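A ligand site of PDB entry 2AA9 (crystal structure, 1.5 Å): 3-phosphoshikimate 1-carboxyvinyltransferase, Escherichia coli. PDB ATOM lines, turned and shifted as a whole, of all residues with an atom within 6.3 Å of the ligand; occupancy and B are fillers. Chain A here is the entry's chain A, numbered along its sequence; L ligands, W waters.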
ATOM      1  N   LYS A  22      28.138  24.746  13.313  1.00  0.00           N
ATOM      2  CA  LYS A  22      27.988  23.296  13.486  1.00  0.00           C
ATOM      3  C   LYS A  22      26.551  22.917  13.794  1.00  0.00           C
ATOM      4  O   LYS A  22      26.006  21.993  13.177  1.00  0.00           O
ATOM      5  CB  LYS A  22      28.900  22.794  14.609  1.00  0.00           C
ATOM      6  CG  LYS A  22      28.752  21.312  14.931  1.00  0.00           C
ATOM      7  CD  LYS A  22      28.102  21.121  16.324  1.00  0.00           C
ATOM      8  CE  LYS A  22      29.087  21.467  17.449  1.00  0.00           C
ATOM      9  NZ  LYS A  22      28.434  21.516  18.799  1.00  0.00           N
ATOM     10  N   SER A  23      25.921  23.645  14.722  1.00  0.00           N
ATOM     11  CA  SER A  23      24.531  23.367  15.123  1.00  0.00           C
ATOM     12  C   SER A  23      23.584  23.464  13.949  1.00  0.00           C
ATOM     13  O   SER A  23      22.718  22.609  13.779  1.00  0.00           O
ATOM     14  CB  SER A  23      24.103  24.339  16.204  1.00  0.00           C
ATOM     15  OG  SER A  23      24.860  24.121  17.391  1.00  0.00           O
ATOM     16  N   VAL A  24      23.736  24.520  13.157  1.00  0.00           N
ATOM     17  CA  VAL A  24      22.875  24.696  11.990  1.00  0.00           C
ATOM     18  C   VAL A  24      23.193  23.685  10.896  1.00  0.00           C
ATOM     19  O   VAL A  24      22.295  23.099  10.306  1.00  0.00           O
ATOM     20  CB  VAL A  24      22.996  26.131  11.428  1.00  0.00           C
ATOM     21  CG1 VAL A  24      22.185  26.256  10.132  1.00  0.00           C
ATOM     22  CG2 VAL A  24      22.519  27.144  12.502  1.00  0.00           C
ATOM     23  N   ARG A  27      21.823  20.110  11.601  1.00  0.00           N
ATOM     24  CA  ARG A  27      20.361  20.089  11.543  1.00  0.00           C
ATOM     25  C   ARG A  27      19.923  20.204  10.072  1.00  0.00           C
ATOM     26  O   ARG A  27      19.030  19.486   9.601  1.00  0.00           O
ATOM     27  CB  ARG A  27      19.752  21.282  12.296  1.00  0.00           C
ATOM     28  CG  ARG A  27      19.686  21.128  13.837  1.00  0.00           C
ATOM     29  CD  ARG A  27      19.440  22.479  14.470  1.00  0.00           C
ATOM     30  NE  ARG A  27      19.221  22.438  15.926  1.00  0.00           N
ATOM     31  CZ  ARG A  27      20.175  22.294  16.835  1.00  0.00           C
ATOM     32  NH1 ARG A  27      19.871  22.312  18.129  1.00  0.00           N
ATOM     33  NH2 ARG A  27      21.440  22.123  16.468  1.00  0.00           N
ATOM     34  N   THR A  97      25.384  16.343  17.879  1.00  0.00           N
ATOM     35  CA  THR A  97      24.374  16.805  16.929  1.00  0.00           C
ATOM     36  C   THR A  97      24.121  15.813  15.794  1.00  0.00           C
ATOM     37  O   THR A  97      23.282  16.057  14.927  1.00  0.00           O
ATOM     38  CB  THR A  97      24.704  18.193  16.356  1.00  0.00           C
ATOM     39  OG1 THR A  97      25.925  18.145  15.605  1.00  0.00           O
ATOM     40  CG2 THR A  97      24.826  19.218  17.475  1.00  0.00           C
ATOM     41  N   ARG A 100      22.348  12.395  18.794  1.00  0.00           N
ATOM     42  CA  ARG A 100      21.008  12.548  19.336  1.00  0.00           C
ATOM     43  C   ARG A 100      19.941  12.669  18.234  1.00  0.00           C
ATOM     44  O   ARG A 100      18.942  11.938  18.274  1.00  0.00           O
ATOM     45  CB  ARG A 100      20.964  13.737  20.295  1.00  0.00           C
ATOM     46  CG  ARG A 100      21.479  13.417  21.702  1.00  0.00           C
ATOM     47  CD  ARG A 100      22.996  13.071  21.729  1.00  0.00           C
ATOM     48  NE  ARG A 100      23.471  12.914  23.105  1.00  0.00           N
ATOM     49  CZ  ARG A 100      23.929  13.902  23.883  1.00  0.00           C
ATOM     50  NH1 ARG A 100      24.310  13.640  25.111  1.00  0.00           N
ATOM     51  NH2 ARG A 100      23.985  15.150  23.441  1.00  0.00           N
ATOM     52  N   ARG A 124      28.442   9.780  27.289  1.00  0.00           N
ATOM     53  CA  ARG A 124      27.587  10.976  27.236  1.00  0.00           C
ATOM     54  C   ARG A 124      26.153  10.453  27.255  1.00  0.00           C
ATOM     55  O   ARG A 124      25.760   9.632  26.430  1.00  0.00           O
ATOM     56  CB  ARG A 124      27.916  11.797  25.993  1.00  0.00           C
ATOM     57  CG  ARG A 124      29.300  12.461  26.125  1.00  0.00           C
ATOM     58  CD  ARG A 124      29.739  13.210  24.910  1.00  0.00           C
ATOM     59  NE  ARG A 124      28.878  14.349  24.616  1.00  0.00           N
ATOM     60  CZ  ARG A 124      28.962  15.041  23.486  1.00  0.00           C
ATOM     61  NH1 ARG A 124      28.139  16.064  23.273  1.00  0.00           N
ATOM     62  NH2 ARG A 124      29.868  14.721  22.576  1.00  0.00           N
ATOM     63  N   SER A 169      19.908  17.883  29.027  1.00  0.00           N
ATOM     64  CA  SER A 169      20.311  18.296  27.689  1.00  0.00           C
ATOM     65  C   SER A 169      19.138  18.786  26.840  1.00  0.00           C
ATOM     66  O   SER A 169      18.062  18.185  26.870  1.00  0.00           O
ATOM     67  CB  SER A 169      20.936  17.104  26.942  1.00  0.00           C
ATOM     68  OG  SER A 169      21.114  17.384  25.564  1.00  0.00           O
ATOM     69  N   SER A 170      19.346  19.841  26.062  1.00  0.00           N
ATOM     70  CA  SER A 170      18.302  20.318  25.168  1.00  0.00           C
ATOM     71  C   SER A 170      18.273  19.459  23.907  1.00  0.00           C
ATOM     72  O   SER A 170      17.302  19.501  23.142  1.00  0.00           O
ATOM     73  CB  SER A 170      18.578  21.764  24.754  1.00  0.00           C
ATOM     74  OG  SER A 170      19.775  21.880  23.976  1.00  0.00           O
ATOM     75  N   GLN A 171      19.323  18.684  23.671  1.00  0.00           N
ATOM     76  CA  GLN A 171      19.412  17.901  22.450  1.00  0.00           C
ATOM     77  C   GLN A 171      18.387  16.781  22.361  1.00  0.00           C
ATOM     78  O   GLN A 171      18.049  16.351  21.262  1.00  0.00           O
ATOM     79  CB  GLN A 171      20.820  17.336  22.300  1.00  0.00           C
ATOM     80  CG  GLN A 171      21.879  18.402  22.051  1.00  0.00           C
ATOM     81  CD  GLN A 171      23.258  17.823  21.882  1.00  0.00           C
ATOM     82  OE1 GLN A 171      23.424  16.799  21.222  1.00  0.00           O
ATOM     83  NE2 GLN A 171      24.260  18.486  22.449  1.00  0.00           N
ATOM     84  N   THR A 174      15.390  18.509  21.027  1.00  0.00           N
ATOM     85  CA  THR A 174      15.660  18.838  19.627  1.00  0.00           C
ATOM     86  C   THR A 174      15.459  17.616  18.735  1.00  0.00           C
ATOM     87  O   THR A 174      14.823  17.712  17.689  1.00  0.00           O
ATOM     88  CB  THR A 174      17.113  19.358  19.456  1.00  0.00           C
ATOM     89  OG1 THR A 174      17.122  20.751  19.808  1.00  0.00           O
ATOM     90  CG2 THR A 174      17.651  19.151  18.021  1.00  0.00           C
ATOM     91  N   SER A 197      19.425  25.245  28.416  1.00  0.00           N
ATOM     92  CA  SER A 197      19.894  25.814  27.144  1.00  0.00           C
ATOM     93  C   SER A 197      18.828  25.929  26.026  1.00  0.00           C
ATOM     94  O   SER A 197      19.027  25.473  24.894  1.00  0.00           O
ATOM     95  CB  SER A 197      21.114  24.993  26.687  1.00  0.00           C
ATOM     96  OG  SER A 197      22.030  24.878  27.781  1.00  0.00           O
ATOM     97  N   TYR A 200      18.892  26.553  21.895  1.00  0.00           N
ATOM     98  CA  TYR A 200      19.095  25.508  20.900  1.00  0.00           C
ATOM     99  C   TYR A 200      17.792  24.931  20.389  1.00  0.00           C
ATOM    100  O   TYR A 200      17.737  24.410  19.288  1.00  0.00           O
ATOM    101  CB  TYR A 200      20.011  24.409  21.443  1.00  0.00           C
ATOM    102  CG  TYR A 200      21.436  24.870  21.574  1.00  0.00           C
ATOM    103  CD1 TYR A 200      21.957  25.310  22.809  1.00  0.00           C
ATOM    104  CD2 TYR A 200      22.271  24.900  20.455  1.00  0.00           C
ATOM    105  CE1 TYR A 200      23.263  25.765  22.912  1.00  0.00           C
ATOM    106  CE2 TYR A 200      23.603  25.366  20.553  1.00  0.00           C
ATOM    107  CZ  TYR A 200      24.071  25.802  21.782  1.00  0.00           C
ATOM    108  OH  TYR A 200      25.366  26.249  21.933  1.00  0.00           O
ATOM    109  N   ILE A 203      16.813  27.238  17.707  1.00  0.00           N
ATOM    110  CA  ILE A 203      17.535  26.951  16.469  1.00  0.00           C
ATOM    111  C   ILE A 203      16.827  25.813  15.723  1.00  0.00           C
ATOM    112  O   ILE A 203      16.602  25.885  14.515  1.00  0.00           O
ATOM    113  CB  ILE A 203      19.012  26.502  16.768  1.00  0.00           C
ATOM    114  CG1 ILE A 203      19.810  27.671  17.351  1.00  0.00           C
ATOM    115  CG2 ILE A 203      19.653  25.991  15.482  1.00  0.00           C
ATOM    116  CD1 ILE A 203      21.261  27.323  17.641  1.00  0.00           C
ATOM    117  N   THR A 204      16.453  24.762  16.449  1.00  0.00           N
ATOM    118  CA  THR A 204      15.761  23.617  15.860  1.00  0.00           C
ATOM    119  C   THR A 204      14.439  24.010  15.198  1.00  0.00           C
ATOM    120  O   THR A 204      14.151  23.580  14.080  1.00  0.00           O
ATOM    121  CB  THR A 204      15.523  22.566  16.937  1.00  0.00           C
ATOM    122  OG1 THR A 204      16.806  22.151  17.425  1.00  0.00           O
ATOM    123  CG2 THR A 204      14.789  21.343  16.372  1.00  0.00           C
ATOM    124  N   PRO A 312      26.131  27.854  27.201  1.00  0.00           N
ATOM    125  CA  PRO A 312      27.140  26.957  27.763  1.00  0.00           C
ATOM    126  C   PRO A 312      28.449  26.808  27.021  1.00  0.00           C
ATOM    127  O   PRO A 312      29.506  26.706  27.661  1.00  0.00           O
ATOM    128  CB  PRO A 312      26.388  25.634  27.916  1.00  0.00           C
ATOM    129  CG  PRO A 312      25.359  25.677  26.805  1.00  0.00           C
ATOM    130  CD  PRO A 312      24.898  27.118  26.854  1.00  0.00           C
ATOM    131  N   ASP A 313      28.398  26.792  25.688  1.00  0.00           N
ATOM    132  CA  ASP A 313      29.621  26.593  24.918  1.00  0.00           C
ATOM    133  C   ASP A 313      30.484  27.852  24.892  1.00  0.00           C
ATOM    134  O   ASP A 313      31.654  27.807  25.269  1.00  0.00           O
ATOM    135  CB  ASP A 313      29.268  26.146  23.496  1.00  0.00           C
ATOM    136  CG  ASP A 313      28.630  24.761  23.428  1.00  0.00           C
ATOM    137  OD1 ASP A 313      28.219  24.376  22.321  1.00  0.00           O
ATOM    138  OD2 ASP A 313      28.519  24.052  24.465  1.00  0.00           O
ATOM    139  N   ASN A 336      25.724  21.229  33.128  1.00  0.00           N
ATOM    140  CA  ASN A 336      25.784  20.542  31.837  1.00  0.00           C
ATOM    141  C   ASN A 336      27.179  20.494  31.232  1.00  0.00           C
ATOM    142  O   ASN A 336      27.447  19.653  30.352  1.00  0.00           O
ATOM    143  CB  ASN A 336      24.739  21.130  30.846  1.00  0.00           C
ATOM    144  CG  ASN A 336      24.851  22.644  30.649  1.00  0.00           C
ATOM    145  OD1 ASN A 336      25.465  23.347  31.447  1.00  0.00           O
ATOM    146  ND2 ASN A 336      24.223  23.143  29.592  1.00  0.00           N
ATOM    147  N   LYS A 340      29.519  17.007  28.450  1.00  0.00           N
ATOM    148  CA  LYS A 340      29.836  17.319  27.058  1.00  0.00           C
ATOM    149  C   LYS A 340      31.104  16.648  26.516  1.00  0.00           C
ATOM    150  O   LYS A 340      31.400  15.529  26.922  1.00  0.00           O
ATOM    151  CB  LYS A 340      29.835  18.834  26.918  1.00  0.00           C
ATOM    152  CG  LYS A 340      28.425  19.389  27.194  1.00  0.00           C
ATOM    153  CD  LYS A 340      28.355  20.897  27.089  1.00  0.00           C
ATOM    154  CE  LYS A 340      26.950  21.409  27.424  1.00  0.00           C
ATOM    155  NZ  LYS A 340      25.910  20.964  26.461  1.00  0.00           N
ATOM    156  N   GLU A 341      31.848  17.301  25.608  1.00  0.00           N
ATOM    157  CA  GLU A 341      33.023  16.664  25.013  1.00  0.00           C
ATOM    158  C   GLU A 341      33.949  16.055  26.064  1.00  0.00           C
ATOM    159  O   GLU A 341      34.600  15.028  25.807  1.00  0.00           O
ATOM    160  CB  GLU A 341      33.768  17.640  24.092  1.00  0.00           C
ATOM    161  CG  GLU A 341      33.111  17.777  22.694  1.00  0.00           C
ATOM    162  CD  GLU A 341      31.900  18.740  22.637  1.00  0.00           C
ATOM    163  OE1 GLU A 341      31.195  18.982  23.667  1.00  0.00           O
ATOM    164  OE2 GLU A 341      31.657  19.243  21.539  1.00  0.00           O
ATOM    165  N   ARG A 344      33.769  19.521  31.381  1.00  0.00           N
ATOM    166  CA  ARG A 344      34.400  20.827  31.244  1.00  0.00           C
ATOM    167  C   ARG A 344      34.611  21.594  32.541  1.00  0.00           C
ATOM    168  O   ARG A 344      35.484  22.455  32.594  1.00  0.00           O
ATOM    169  CB  ARG A 344      33.636  21.659  30.208  1.00  0.00           C
ATOM    170  CG  ARG A 344      33.811  21.072  28.793  1.00  0.00           C
ATOM    171  CD  ARG A 344      32.771  21.587  27.798  1.00  0.00           C
ATOM    172  NE  ARG A 344      33.286  21.395  26.439  1.00  0.00           N
ATOM    173  CZ  ARG A 344      32.610  21.675  25.325  1.00  0.00           C
ATOM    174  NH1 ARG A 344      33.173  21.502  24.136  1.00  0.00           N
ATOM    175  NH2 ARG A 344      31.342  22.087  25.401  1.00  0.00           N
ATOM    176  N   ARG A 386      37.106  22.939  22.335  1.00  0.00           N
ATOM    177  CA  ARG A 386      36.987  24.205  23.053  1.00  0.00           C
ATOM    178  C   ARG A 386      38.044  24.428  24.134  1.00  0.00           C
ATOM    179  O   ARG A 386      38.362  25.577  24.466  1.00  0.00           O
ATOM    180  CB  ARG A 386      35.566  24.346  23.633  1.00  0.00           C
ATOM    181  CG  ARG A 386      34.517  24.400  22.524  1.00  0.00           C
ATOM    182  CD  ARG A 386      33.194  25.084  22.963  1.00  0.00           C
ATOM    183  NE  ARG A 386      32.228  24.830  21.891  1.00  0.00           N
ATOM    184  CZ  ARG A 386      32.255  25.398  20.684  1.00  0.00           C
ATOM    185  NH1 ARG A 386      31.348  25.030  19.768  1.00  0.00           N
ATOM    186  NH2 ARG A 386      33.104  26.394  20.399  1.00  0.00           N
HETATM  187  O1  LIG L   1      26.331  22.430  24.276  1.00  0.00           O
HETATM  188  C1  LIG L   1      25.581  22.505  23.073  1.00  0.00           C
HETATM  189  C2  LIG L   1      26.129  21.583  21.994  1.00  0.00           C
HETATM  190  O2  LIG L   1      27.508  21.898  21.736  1.00  0.00           O
HETATM  191  C3  LIG L   1      25.292  21.787  20.725  1.00  0.00           C
HETATM  192  C4  LIG L   1      23.867  21.851  20.875  1.00  0.00           C
HETATM  193  C5  LIG L   1      22.958  21.773  19.656  1.00  0.00           C
HETATM  194  O3  LIG L   1      21.790  21.358  19.840  1.00  0.00           O
HETATM  195  O4  LIG L   1      23.357  22.177  18.565  1.00  0.00           O
HETATM  196  C6  LIG L   1      23.273  22.043  22.145  1.00  0.00           C
HETATM  197  C7  LIG L   1      24.107  22.131  23.398  1.00  0.00           C
HETATM  198  O5  LIG L   1      24.046  20.906  24.104  1.00  0.00           O
HETATM  199  O   HOH W   1      19.434  21.053  21.283  1.00  0.00           O
HETATM  200  O   HOH W   2      28.637  20.033  23.813  1.00  0.00           O
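NH1 of Arg 27 lies within salt-bridge range of O3 of the ligand (2.7 Å).
The side-chain amino group (NZ) of Lys 340 sits at hydrogen-bond distance from an oxygen (O1) of the ligand (2.7 Å).
An oxygen (O2) of the ligand is in hydrogen-bond range of the side-chain carboxylate (OD1) of Asp 313 (2.6 Å).
O5 of the ligand sits at hydrogen-bond distance from NE2 of Gln 171.
The side-chain amino group (NZ) of Lys 22 lies within hydrogen-bond range of an oxygen (O2) of the ligand (3.1 Å).
O4 of the ligand is in hydrogen-bond range of OG of Ser 23 (2.7 Å).
Water W1 lies within hydrogen-bond range of the side-chain hydroxyl (OG1) of Thr 174, an oxygen (O3) of the ligand, the side-chain hydroxyl (OG) of Ser 170, the backbone NH (N) of Gln 171 and the guanidinium group (NH1) of Arg 27.
Water W2 bridges OE1 of Glu 341 (2.8 Å) and O2 of the ligand (3.0 Å).
NE of Arg 27 is in hydrogen-bond range of OG1 of Thr 204 (2.9 Å).
The side-chain amide oxygen (OE1) of Gln 171 lies within hydrogen-bond range of the guanidinium group (NH2) of Arg 100 (2.8 Å).
The guanidinium group (NH1) of Arg 27 is in hydrogen-bond range of the backbone carbonyl oxygen (O) of Tyr 200, 3.2 Å away.
The side-chain hydroxyl of Tyr 200 lies within hydrogen-bond range of the side-chain carboxylate of Asp 313 (3.4 Å).
The side-chain hydroxyl of Thr 204 lies within hydrogen-bond range of the backbone carbonyl oxygen of Tyr 200, at 3.1 Å.
The side-chain hydroxyl of Ser 169 is in hydrogen-bond range of the backbone NH of Gln 171 (2.9 Å).
The side-chain carboxylate (OD2) of Asp 313 is in salt-bridge range of the guanidinium group (NH2) of Arg 344.
O of Ser 23 is in hydrogen-bond range of NH2 of Arg 27 (3.0 Å).
Thr 97 touches the ligand.
Ser 170 touches the ligand.
Tyr 200 touches the ligand.
Of the 22 residues printed, 9 come within 4 Å of the ligand.
The nearest printed residue that does not touch the ligand is Pro 312 (4.2 Å).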
